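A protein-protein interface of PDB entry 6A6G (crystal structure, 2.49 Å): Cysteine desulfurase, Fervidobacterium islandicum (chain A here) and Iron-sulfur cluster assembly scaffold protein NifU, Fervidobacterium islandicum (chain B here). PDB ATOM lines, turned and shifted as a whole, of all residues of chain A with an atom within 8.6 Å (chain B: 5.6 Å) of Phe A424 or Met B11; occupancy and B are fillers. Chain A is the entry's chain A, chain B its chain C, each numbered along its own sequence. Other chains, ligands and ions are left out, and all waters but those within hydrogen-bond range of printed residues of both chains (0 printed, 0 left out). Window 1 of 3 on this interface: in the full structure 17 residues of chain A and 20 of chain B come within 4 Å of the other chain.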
ATOM      1  N   VAL A 350      -9.340  31.732 -23.918  1.00  0.00           N
ATOM      2  CA  VAL A 350      -8.711  31.849 -22.627  1.00  0.00           C
ATOM      3  C   VAL A 350      -7.896  33.132 -22.632  1.00  0.00           C
ATOM      4  O   VAL A 350      -7.211  33.404 -23.623  1.00  0.00           O
ATOM      5  CB  VAL A 350      -7.832  30.630 -22.331  1.00  0.00           C
ATOM      6  CG1 VAL A 350      -7.037  30.873 -21.056  1.00  0.00           C
ATOM      7  CG2 VAL A 350      -8.714  29.364 -22.217  1.00  0.00           C
ATOM      8  N   LYS A 351      -8.032  33.956 -21.583  1.00  0.00           N
ATOM      9  CA  LYS A 351      -7.325  35.252 -21.522  1.00  0.00           C
ATOM     10  C   LYS A 351      -5.828  34.986 -21.672  1.00  0.00           C
ATOM     11  O   LYS A 351      -5.272  34.268 -20.883  1.00  0.00           O
ATOM     12  CB  LYS A 351      -7.570  35.987 -20.189  1.00  0.00           C
ATOM     13  CG  LYS A 351      -8.961  36.621 -20.022  1.00  0.00           C
ATOM     14  CD  LYS A 351      -9.106  37.422 -18.713  1.00  0.00           C
ATOM     15  CE  LYS A 351     -10.541  37.423 -18.164  1.00  0.00           C
ATOM     16  NZ  LYS A 351     -11.535  38.237 -18.917  1.00  0.00           N
ATOM     17  N   GLY A 352      -5.200  35.529 -22.701  1.00  0.00           N
ATOM     18  CA  GLY A 352      -3.761  35.459 -22.830  1.00  0.00           C
ATOM     19  C   GLY A 352      -3.209  34.132 -23.299  1.00  0.00           C
ATOM     20  O   GLY A 352      -2.016  33.892 -23.162  1.00  0.00           O
ATOM     21  N   VAL A 353      -4.060  33.262 -23.842  1.00  0.00           N
ATOM     22  CA  VAL A 353      -3.594  31.979 -24.397  1.00  0.00           C
ATOM     23  C   VAL A 353      -4.255  31.782 -25.728  1.00  0.00           C
ATOM     24  O   VAL A 353      -5.466  31.858 -25.829  1.00  0.00           O
ATOM     25  CB  VAL A 353      -3.921  30.792 -23.478  1.00  0.00           C
ATOM     26  CG1 VAL A 353      -3.301  29.511 -24.033  1.00  0.00           C
ATOM     27  CG2 VAL A 353      -3.424  31.069 -22.055  1.00  0.00           C
ATOM     28  N   HIS A 354      -3.443  31.592 -26.748  1.00  0.00           N
ATOM     29  CA  HIS A 354      -3.933  31.367 -28.113  1.00  0.00           C
ATOM     30  C   HIS A 354      -4.696  30.041 -28.250  1.00  0.00           C
ATOM     31  O   HIS A 354      -4.326  29.023 -27.642  1.00  0.00           O
ATOM     32  CB  HIS A 354      -2.767  31.400 -29.106  1.00  0.00           C
ATOM     33  CG  HIS A 354      -3.180  31.515 -30.540  1.00  0.00           C
ATOM     34  ND1 HIS A 354      -3.540  30.426 -31.302  1.00  0.00           N
ATOM     35  CD2 HIS A 354      -3.217  32.581 -31.378  1.00  0.00           C
ATOM     36  CE1 HIS A 354      -3.817  30.821 -32.538  1.00  0.00           C
ATOM     37  NE2 HIS A 354      -3.613  32.120 -32.619  1.00  0.00           N
ATOM     38  N   HIS A 356      -4.818  27.681 -30.419  1.00  0.00           N
ATOM     39  CA  HIS A 356      -4.054  26.441 -30.714  1.00  0.00           C
ATOM     40  C   HIS A 356      -3.421  25.827 -29.497  1.00  0.00           C
ATOM     41  O   HIS A 356      -3.469  24.611 -29.309  1.00  0.00           O
ATOM     42  CB  HIS A 356      -2.970  26.661 -31.722  1.00  0.00           C
ATOM     43  CG  HIS A 356      -3.465  27.220 -33.004  1.00  0.00           C
ATOM     44  ND1 HIS A 356      -2.617  27.616 -34.012  1.00  0.00           N
ATOM     45  CD2 HIS A 356      -4.723  27.505 -33.421  1.00  0.00           C
ATOM     46  CE1 HIS A 356      -3.334  28.087 -35.010  1.00  0.00           C
ATOM     47  NE2 HIS A 356      -4.616  28.019 -34.681  1.00  0.00           N
ATOM     48  N   ASP A 357      -2.867  26.661 -28.634  1.00  0.00           N
ATOM     49  CA  ASP A 357      -2.211  26.137 -27.461  1.00  0.00           C
ATOM     50  C   ASP A 357      -3.224  25.552 -26.511  1.00  0.00           C
ATOM     51  O   ASP A 357      -2.996  24.502 -25.925  1.00  0.00           O
ATOM     52  CB  ASP A 357      -1.360  27.241 -26.824  1.00  0.00           C
ATOM     53  CG  ASP A 357      -0.322  27.809 -27.811  1.00  0.00           C
ATOM     54  OD1 ASP A 357       0.363  27.038 -28.495  1.00  0.00           O
ATOM     55  OD2 ASP A 357      -0.199  29.044 -27.916  1.00  0.00           O
ATOM     56  N   VAL A 358      -4.353  26.224 -26.366  1.00  0.00           N
ATOM     57  CA  VAL A 358      -5.467  25.724 -25.536  1.00  0.00           C
ATOM     58  C   VAL A 358      -5.946  24.364 -26.021  1.00  0.00           C
ATOM     59  O   VAL A 358      -6.060  23.433 -25.241  1.00  0.00           O
ATOM     60  CB  VAL A 358      -6.669  26.694 -25.517  1.00  0.00           C
ATOM     61  CG1 VAL A 358      -7.803  26.126 -24.696  1.00  0.00           C
ATOM     62  CG2 VAL A 358      -6.248  28.036 -24.933  1.00  0.00           C
ATOM     63  N   SER A 359      -6.218  24.237 -27.308  1.00  0.00           N
ATOM     64  CA  SER A 359      -6.683  22.921 -27.821  1.00  0.00           C
ATOM     65  C   SER A 359      -5.590  21.827 -27.774  1.00  0.00           C
ATOM     66  O   SER A 359      -5.882  20.665 -27.534  1.00  0.00           O
ATOM     67  CB  SER A 359      -7.273  23.051 -29.220  1.00  0.00           C
ATOM     68  OG  SER A 359      -8.493  23.756 -29.212  1.00  0.00           O
ATOM     69  N   HIS A 360      -4.331  22.204 -27.978  1.00  0.00           N
ATOM     70  CA  HIS A 360      -3.244  21.222 -27.953  1.00  0.00           C
ATOM     71  C   HIS A 360      -3.111  20.605 -26.587  1.00  0.00           C
ATOM     72  O   HIS A 360      -3.108  19.374 -26.445  1.00  0.00           O
ATOM     73  CB  HIS A 360      -1.926  21.857 -28.350  1.00  0.00           C
ATOM     74  CG  HIS A 360      -0.842  20.862 -28.545  1.00  0.00           C
ATOM     75  ND1 HIS A 360      -0.292  20.603 -29.776  1.00  0.00           N
ATOM     76  CD2 HIS A 360      -0.235  20.019 -27.672  1.00  0.00           C
ATOM     77  CE1 HIS A 360       0.608  19.642 -29.659  1.00  0.00           C
ATOM     78  NE2 HIS A 360       0.650  19.256 -28.397  1.00  0.00           N
ATOM     79  N   ILE A 361      -3.026  21.447 -25.564  1.00  0.00           N
ATOM     80  CA  ILE A 361      -2.890  20.945 -24.192  1.00  0.00           C
ATOM     81  C   ILE A 361      -4.110  20.177 -23.770  1.00  0.00           C
ATOM     82  O   ILE A 361      -3.999  19.120 -23.169  1.00  0.00           O
ATOM     83  CB  ILE A 361      -2.598  22.073 -23.196  1.00  0.00           C
ATOM     84  CG1 ILE A 361      -1.140  22.489 -23.360  1.00  0.00           C
ATOM     85  CG2 ILE A 361      -2.847  21.629 -21.752  1.00  0.00           C
ATOM     86  CD1 ILE A 361      -0.801  23.839 -22.759  1.00  0.00           C
ATOM     87  N   LEU A 362      -5.280  20.719 -24.074  1.00  0.00           N
ATOM     88  CA  LEU A 362      -6.535  20.031 -23.825  1.00  0.00           C
ATOM     89  C   LEU A 362      -6.453  18.625 -24.409  1.00  0.00           C
ATOM     90  O   LEU A 362      -6.815  17.645 -23.771  1.00  0.00           O
ATOM     91  CB  LEU A 362      -7.703  20.820 -24.434  1.00  0.00           C
ATOM     92  CG  LEU A 362      -8.322  21.932 -23.613  1.00  0.00           C
ATOM     93  CD1 LEU A 362      -9.511  22.493 -24.358  1.00  0.00           C
ATOM     94  CD2 LEU A 362      -8.757  21.463 -22.228  1.00  0.00           C
ATOM     95  N   GLY A 416      -9.149  21.066 -17.376  1.00  0.00           N
ATOM     96  CA  GLY A 416      -8.143  21.328 -18.351  1.00  0.00           C
ATOM     97  C   GLY A 416      -7.876  22.802 -18.492  1.00  0.00           C
ATOM     98  O   GLY A 416      -6.729  23.241 -18.487  1.00  0.00           O
ATOM     99  N   LEU A 417      -8.935  23.571 -18.625  1.00  0.00           N
ATOM    100  CA  LEU A 417      -8.803  24.990 -18.867  1.00  0.00           C
ATOM    101  C   LEU A 417      -8.177  25.701 -17.670  1.00  0.00           C
ATOM    102  O   LEU A 417      -7.489  26.704 -17.841  1.00  0.00           O
ATOM    103  CB  LEU A 417     -10.162  25.606 -19.206  1.00  0.00           C
ATOM    104  CG  LEU A 417     -10.843  25.196 -20.495  1.00  0.00           C
ATOM    105  CD1 LEU A 417     -12.254  25.769 -20.505  1.00  0.00           C
ATOM    106  CD2 LEU A 417     -10.074  25.674 -21.716  1.00  0.00           C
ATOM    107  N   LYS A 418      -8.411  25.180 -16.470  1.00  0.00           N
ATOM    108  CA  LYS A 418      -7.786  25.731 -15.242  1.00  0.00           C
ATOM    109  C   LYS A 418      -6.278  25.456 -15.232  1.00  0.00           C
ATOM    110  O   LYS A 418      -5.476  26.352 -14.905  1.00  0.00           O
ATOM    111  CB  LYS A 418      -8.446  25.177 -13.998  1.00  0.00           C
ATOM    112  CG  LYS A 418      -9.754  25.867 -13.720  1.00  0.00           C
ATOM    113  CD  LYS A 418     -10.582  25.109 -12.713  1.00  0.00           C
ATOM    114  CE  LYS A 418     -11.861  25.857 -12.418  1.00  0.00           C
ATOM    115  NZ  LYS A 418     -12.758  25.044 -11.560  1.00  0.00           N
ATOM    116  N   TYR A 419      -5.906  24.241 -15.647  1.00  0.00           N
ATOM    117  CA  TYR A 419      -4.503  23.855 -15.781  1.00  0.00           C
ATOM    118  C   TYR A 419      -3.823  24.767 -16.800  1.00  0.00           C
ATOM    119  O   TYR A 419      -2.711  25.244 -16.584  1.00  0.00           O
ATOM    120  CB  TYR A 419      -4.404  22.372 -16.155  1.00  0.00           C
ATOM    121  CG  TYR A 419      -3.033  21.892 -16.471  1.00  0.00           C
ATOM    122  CD1 TYR A 419      -2.502  22.081 -17.726  1.00  0.00           C
ATOM    123  CD2 TYR A 419      -2.256  21.252 -15.515  1.00  0.00           C
ATOM    124  CE1 TYR A 419      -1.225  21.646 -18.052  1.00  0.00           C
ATOM    125  CE2 TYR A 419      -0.971  20.811 -15.817  1.00  0.00           C
ATOM    126  CZ  TYR A 419      -0.456  21.007 -17.097  1.00  0.00           C
ATOM    127  OH  TYR A 419       0.815  20.587 -17.442  1.00  0.00           O
ATOM    128  N   ILE A 420      -4.522  25.055 -17.892  1.00  0.00           N
ATOM    129  CA  ILE A 420      -3.947  25.841 -18.965  1.00  0.00           C
ATOM    130  C   ILE A 420      -3.734  27.294 -18.535  1.00  0.00           C
ATOM    131  O   ILE A 420      -2.748  27.914 -18.919  1.00  0.00           O
ATOM    132  CB  ILE A 420      -4.838  25.751 -20.210  1.00  0.00           C
ATOM    133  CG1 ILE A 420      -4.692  24.363 -20.836  1.00  0.00           C
ATOM    134  CG2 ILE A 420      -4.487  26.816 -21.234  1.00  0.00           C
ATOM    135  CD1 ILE A 420      -5.763  24.020 -21.860  1.00  0.00           C
ATOM    136  N   ARG A 421      -4.661  27.839 -17.751  1.00  0.00           N
ATOM    137  CA  ARG A 421      -4.508  29.202 -17.255  1.00  0.00           C
ATOM    138  C   ARG A 421      -3.214  29.368 -16.428  1.00  0.00           C
ATOM    139  O   ARG A 421      -2.484  30.331 -16.645  1.00  0.00           O
ATOM    140  CB  ARG A 421      -5.703  29.606 -16.406  1.00  0.00           C
ATOM    141  CG  ARG A 421      -5.714  31.077 -16.073  1.00  0.00           C
ATOM    142  CD  ARG A 421      -6.116  31.279 -14.628  1.00  0.00           C
ATOM    143  NE  ARG A 421      -6.505  32.677 -14.369  1.00  0.00           N
ATOM    144  CZ  ARG A 421      -7.314  33.076 -13.377  1.00  0.00           C
ATOM    145  NH1 ARG A 421      -7.852  32.195 -12.523  1.00  0.00           N
ATOM    146  NH2 ARG A 421      -7.599  34.366 -13.235  1.00  0.00           N
ATOM    147  N   ARG A 422      -2.969  28.444 -15.487  1.00  0.00           N
ATOM    148  CA  ARG A 422      -1.675  28.325 -14.786  1.00  0.00           C
ATOM    149  C   ARG A 422      -0.420  28.068 -15.661  1.00  0.00           C
ATOM    150  O   ARG A 422       0.634  28.633 -15.382  1.00  0.00           O
ATOM    151  CB  ARG A 422      -1.736  27.249 -13.708  1.00  0.00           C
ATOM    152  CG  ARG A 422      -2.582  27.643 -12.509  1.00  0.00           C
ATOM    153  CD  ARG A 422      -2.574  26.582 -11.417  1.00  0.00           C
ATOM    154  NE  ARG A 422      -1.229  26.035 -11.167  1.00  0.00           N
ATOM    155  CZ  ARG A 422      -0.400  26.379 -10.169  1.00  0.00           C
ATOM    156  NH1 ARG A 422      -0.740  27.291  -9.261  1.00  0.00           N
ATOM    157  NH2 ARG A 422       0.793  25.793 -10.079  1.00  0.00           N
ATOM    158  N   TRP A 423      -0.505  27.233 -16.693  1.00  0.00           N
ATOM    159  CA  TRP A 423       0.676  26.913 -17.506  1.00  0.00           C
ATOM    160  C   TRP A 423       1.339  28.159 -18.163  1.00  0.00           C
ATOM    161  O   TRP A 423       2.572  28.281 -18.172  1.00  0.00           O
ATOM    162  CB  TRP A 423       0.324  25.863 -18.579  1.00  0.00           C
ATOM    163  CG  TRP A 423       1.522  25.466 -19.417  1.00  0.00           C
ATOM    164  CD1 TRP A 423       1.785  25.842 -20.707  1.00  0.00           C
ATOM    165  CD2 TRP A 423       2.644  24.674 -18.993  1.00  0.00           C
ATOM    166  NE1 TRP A 423       2.998  25.335 -21.111  1.00  0.00           N
ATOM    167  CE2 TRP A 423       3.547  24.613 -20.081  1.00  0.00           C
ATOM    168  CE3 TRP A 423       2.970  24.013 -17.801  1.00  0.00           C
ATOM    169  CZ2 TRP A 423       4.750  23.910 -20.018  1.00  0.00           C
ATOM    170  CZ3 TRP A 423       4.172  23.322 -17.731  1.00  0.00           C
ATOM    171  CH2 TRP A 423       5.048  23.277 -18.838  1.00  0.00           C
ATOM    172  N   PHE A 424       0.524  29.058 -18.722  1.00  0.00           N
ATOM    173  CA  PHE A 424       1.008  30.256 -19.399  1.00  0.00           C
ATOM    174  C   PHE A 424       0.995  31.516 -18.513  1.00  0.00           C
ATOM    175  O   PHE A 424       1.296  32.591 -18.997  1.00  0.00           O
ATOM    176  CB  PHE A 424       0.188  30.511 -20.663  1.00  0.00           C
ATOM    177  CG  PHE A 424       0.303  29.419 -21.695  1.00  0.00           C
ATOM    178  CD1 PHE A 424       1.293  29.464 -22.673  1.00  0.00           C
ATOM    179  CD2 PHE A 424      -0.587  28.343 -21.697  1.00  0.00           C
ATOM    180  CE1 PHE A 424       1.397  28.452 -23.619  1.00  0.00           C
ATOM    181  CE2 PHE A 424      -0.491  27.342 -22.639  1.00  0.00           C
ATOM    182  CZ  PHE A 424       0.510  27.384 -23.593  1.00  0.00           C
ATOM    183  N   GLU A 425       0.650  31.393 -17.228  1.00  0.00           N
ATOM    184  CA  GLU A 425       0.799  32.507 -16.277  1.00  0.00           C
ATOM    185  C   GLU A 425       2.255  32.948 -16.204  1.00  0.00           C
ATOM    186  O   GLU A 425       2.527  34.144 -16.148  1.00  0.00           O
ATOM    187  CB  GLU A 425       0.314  32.139 -14.864  1.00  0.00           C
ATOM    188  CG  GLU A 425      -1.064  32.682 -14.500  1.00  0.00           C
ATOM    189  CD  GLU A 425      -1.601  32.129 -13.179  1.00  0.00           C
ATOM    190  OE1 GLU A 425      -0.788  31.661 -12.342  1.00  0.00           O
ATOM    191  OE2 GLU A 425      -2.843  32.160 -12.980  1.00  0.00           O
ATOM    192  N   TYR B   6       5.667  21.649 -25.347  1.00  0.00           N
ATOM    193  CA  TYR B   6       6.044  22.976 -24.859  1.00  0.00           C
ATOM    194  C   TYR B   6       7.333  22.921 -23.971  1.00  0.00           C
ATOM    195  O   TYR B   6       7.281  23.027 -22.745  1.00  0.00           O
ATOM    196  CB  TYR B   6       4.859  23.637 -24.115  1.00  0.00           C
ATOM    197  CG  TYR B   6       3.731  23.925 -25.042  1.00  0.00           C
ATOM    198  CD1 TYR B   6       3.812  24.976 -25.958  1.00  0.00           C
ATOM    199  CD2 TYR B   6       2.630  23.108 -25.078  1.00  0.00           C
ATOM    200  CE1 TYR B   6       2.803  25.221 -26.863  1.00  0.00           C
ATOM    201  CE2 TYR B   6       1.617  23.335 -25.977  1.00  0.00           C
ATOM    202  CZ  TYR B   6       1.690  24.388 -26.861  1.00  0.00           C
ATOM    203  OH  TYR B   6       0.645  24.600 -27.718  1.00  0.00           O
ATOM    204  N   SER B   7       8.473  22.764 -24.641  1.00  0.00           N
ATOM    205  CA  SER B   7       9.756  22.606 -24.001  1.00  0.00           C
ATOM    206  C   SER B   7      10.186  23.924 -23.443  1.00  0.00           C
ATOM    207  O   SER B   7       9.616  24.961 -23.779  1.00  0.00           O
ATOM    208  CB  SER B   7      10.805  22.128 -24.988  1.00  0.00           C
ATOM    209  OG  SER B   7      11.168  23.177 -25.871  1.00  0.00           O
ATOM    210  N   GLU B   8      11.209  23.882 -22.601  1.00  0.00           N
ATOM    211  CA  GLU B   8      11.693  25.100 -21.931  1.00  0.00           C
ATOM    212  C   GLU B   8      12.174  26.144 -22.936  1.00  0.00           C
ATOM    213  O   GLU B   8      11.958  27.327 -22.718  1.00  0.00           O
ATOM    214  CB  GLU B   8      12.722  24.831 -20.822  1.00  0.00           C
ATOM    215  CG  GLU B   8      13.244  23.406 -20.679  1.00  0.00           C
ATOM    216  CD  GLU B   8      12.301  22.433 -20.000  1.00  0.00           C
ATOM    217  OE1 GLU B   8      11.582  22.801 -19.058  1.00  0.00           O
ATOM    218  OE2 GLU B   8      12.296  21.274 -20.408  1.00  0.00           O
ATOM    219  N   PHE B   9      12.729  25.694 -24.066  1.00  0.00           N
ATOM    220  CA  PHE B   9      13.229  26.583 -25.104  1.00  0.00           C
ATOM    221  C   PHE B   9      12.064  27.274 -25.817  1.00  0.00           C
ATOM    222  O   PHE B   9      12.065  28.483 -26.032  1.00  0.00           O
ATOM    223  CB  PHE B   9      14.075  25.768 -26.076  1.00  0.00           C
ATOM    224  CG  PHE B   9      14.550  26.523 -27.273  1.00  0.00           C
ATOM    225  CD1 PHE B   9      13.779  26.576 -28.426  1.00  0.00           C
ATOM    226  CD2 PHE B   9      15.795  27.149 -27.272  1.00  0.00           C
ATOM    227  CE1 PHE B   9      14.223  27.251 -29.564  1.00  0.00           C
ATOM    228  CE2 PHE B   9      16.262  27.841 -28.403  1.00  0.00           C
ATOM    229  CZ  PHE B   9      15.469  27.890 -29.552  1.00  0.00           C
ATOM    230  N   ILE B  10      11.055  26.484 -26.149  1.00  0.00           N
ATOM    231  CA  ILE B  10       9.881  26.998 -26.807  1.00  0.00           C
ATOM    232  C   ILE B  10       9.154  27.998 -25.927  1.00  0.00           C
ATOM    233  O   ILE B  10       8.781  29.053 -26.384  1.00  0.00           O
ATOM    234  CB  ILE B  10       8.964  25.856 -27.289  1.00  0.00           C
ATOM    235  CG1 ILE B  10       9.604  25.221 -28.523  1.00  0.00           C
ATOM    236  CG2 ILE B  10       7.566  26.374 -27.610  1.00  0.00           C
ATOM    237  CD1 ILE B  10       8.841  24.038 -29.076  1.00  0.00           C
ATOM    238  N   MET B  11       8.963  27.677 -24.666  1.00  0.00           N
ATOM    239  CA  MET B  11       8.306  28.616 -23.775  1.00  0.00           C
ATOM    240  C   MET B  11       9.114  29.920 -23.660  1.00  0.00           C
ATOM    241  O   MET B  11       8.531  31.007 -23.727  1.00  0.00           O
ATOM    242  CB  MET B  11       8.032  27.976 -22.413  1.00  0.00           C
ATOM    243  CG  MET B  11       6.987  26.867 -22.450  1.00  0.00           C
ATOM    244  SD  MET B  11       5.372  27.324 -23.172  1.00  0.00           S
ATOM    245  CE  MET B  11       4.767  28.311 -21.822  1.00  0.00           C
ATOM    246  N   ASP B  12      10.443  29.824 -23.563  1.00  0.00           N
ATOM    247  CA  ASP B  12      11.289  31.028 -23.401  1.00  0.00           C
ATOM    248  C   ASP B  12      11.183  31.946 -24.614  1.00  0.00           C
ATOM    249  O   ASP B  12      10.967  33.129 -24.459  1.00  0.00           O
ATOM    250  CB  ASP B  12      12.784  30.666 -23.155  1.00  0.00           C
ATOM    251  CG  ASP B  12      13.052  30.127 -21.736  1.00  0.00           C
ATOM    252  OD1 ASP B  12      12.222  30.367 -20.833  1.00  0.00           O
ATOM    253  OD2 ASP B  12      14.096  29.452 -21.519  1.00  0.00           O
ATOM    254  N   TYR B  13      11.342  31.393 -25.813  1.00  0.00           N
ATOM    255  CA  TYR B  13      11.275  32.180 -27.037  1.00  0.00           C
ATOM    256  C   TYR B  13       9.862  32.611 -27.417  1.00  0.00           C
ATOM    257  O   TYR B  13       9.716  33.563 -28.159  1.00  0.00           O
ATOM    258  CB  TYR B  13      11.962  31.474 -28.211  1.00  0.00           C
ATOM    259  CG  TYR B  13      13.471  31.645 -28.217  1.00  0.00           C
ATOM    260  CD1 TYR B  13      14.063  32.744 -28.842  1.00  0.00           C
ATOM    261  CD2 TYR B  13      14.307  30.724 -27.593  1.00  0.00           C
ATOM    262  CE1 TYR B  13      15.445  32.902 -28.859  1.00  0.00           C
ATOM    263  CE2 TYR B  13      15.680  30.886 -27.587  1.00  0.00           C
ATOM    264  CZ  TYR B  13      16.244  31.974 -28.220  1.00  0.00           C
ATOM    265  OH  TYR B  13      17.603  32.134 -28.229  1.00  0.00           O
ATOM    266  N   SER B  14       8.832  31.948 -26.894  1.00  0.00           N
ATOM    267  CA  SER B  14       7.444  32.390 -27.108  1.00  0.00           C
ATOM    268  C   SER B  14       7.125  33.710 -26.390  1.00  0.00           C
ATOM    269  O   SER B  14       6.226  34.421 -26.784  1.00  0.00           O
ATOM    270  CB  SER B  14       6.445  31.330 -26.647  1.00  0.00           C
ATOM    271  OG  SER B  14       6.308  31.348 -25.237  1.00  0.00           O
ATOM    272  N   LYS B  15       7.865  34.020 -25.334  1.00  0.00           N
ATOM    273  CA  LYS B  15       7.592  35.177 -24.497  1.00  0.00           C
ATOM    274  C   LYS B  15       8.434  36.375 -24.898  1.00  0.00           C
ATOM    275  O   LYS B  15       8.317  37.429 -24.298  1.00  0.00           O
ATOM    276  CB  LYS B  15       7.880  34.828 -23.027  1.00  0.00           C
ATOM    277  CG  LYS B  15       6.841  33.916 -22.408  1.00  0.00           C
ATOM    278  CD  LYS B  15       7.341  33.226 -21.154  1.00  0.00           C
ATOM    279  CE  LYS B  15       6.276  32.285 -20.610  1.00  0.00           C
ATOM    280  NZ  LYS B  15       6.855  31.232 -19.721  1.00  0.00           N
ATOM    281  N   ALA B  63       1.934  29.899 -29.313  1.00  0.00           N
ATOM    282  CA  ALA B  63       3.238  29.817 -28.659  1.00  0.00           C
ATOM    283  C   ALA B  63       4.327  29.284 -29.609  1.00  0.00           C
ATOM    284  O   ALA B  63       5.419  29.803 -29.663  1.00  0.00           O
ATOM    285  CB  ALA B  63       3.141  28.956 -27.423  1.00  0.00           C
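Phe A424 touches just one residue of chain B: Met B11 (3.8 Å).
Met B11 touches just these residues of chain A: Trp A423 and Phe A424.
Of the printed residues of chain B, Asp A357 touches Tyr B6 (2.6 Å) and Ala B63 (2.7 Å).
Printed residues of chain B within 4 Å of Ile A361: Tyr B6.
Of the printed residues of chain B, His A360 touches Tyr B6.
Lys B15 touches none of the printed residues of chain A.
The nearest residue of chain B that does not touch Phe A424 is Ala B63 (4.2 Å).
The nearest printed residue of chain B that does not touch Asp A357 is Ser B14 (7.1 Å).
O of Met B11 is in hydrogen-bond range of OG of Ser B14 (2.7 Å).
His A360 touches Tyr B6.
CE2 of Tyr B6 touches CG1 of Ile A361, at 3.9 Å.
Trp A423 touches Tyr B6.
CE of Met B11 touches CD1 of Phe A424, 3.8 Å away.
The side-chain carboxylate of Asp A357 lies within hydrogen-bond range of the side-chain hydroxyl of Tyr B6 (2.6 Å).
OD2 of Asp A357 lies within hydrogen-bond range of N of Ala B63, 2.7 Å away.
NE1 of Trp A423 lies close to SD of Met B11 (3.7 Å).
Of the 22 printed residues of chain A, 5 touch a printed residue of chain B.
Printed residues of chain A that touch a printed residue of chain B: Asp A357, His A360, Ile A361, Trp A423 and Phe A424.
Hydrophobic or aromatic side chains of chain A within 4 Å of the printed part of chain B: His A360, Ile A361, Trp A423 and Phe A424.
Among the printed residues, no Asp or Glu carboxylate lies within 4 Å of a Lys or Arg side-chain nitrogen of the other chain.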
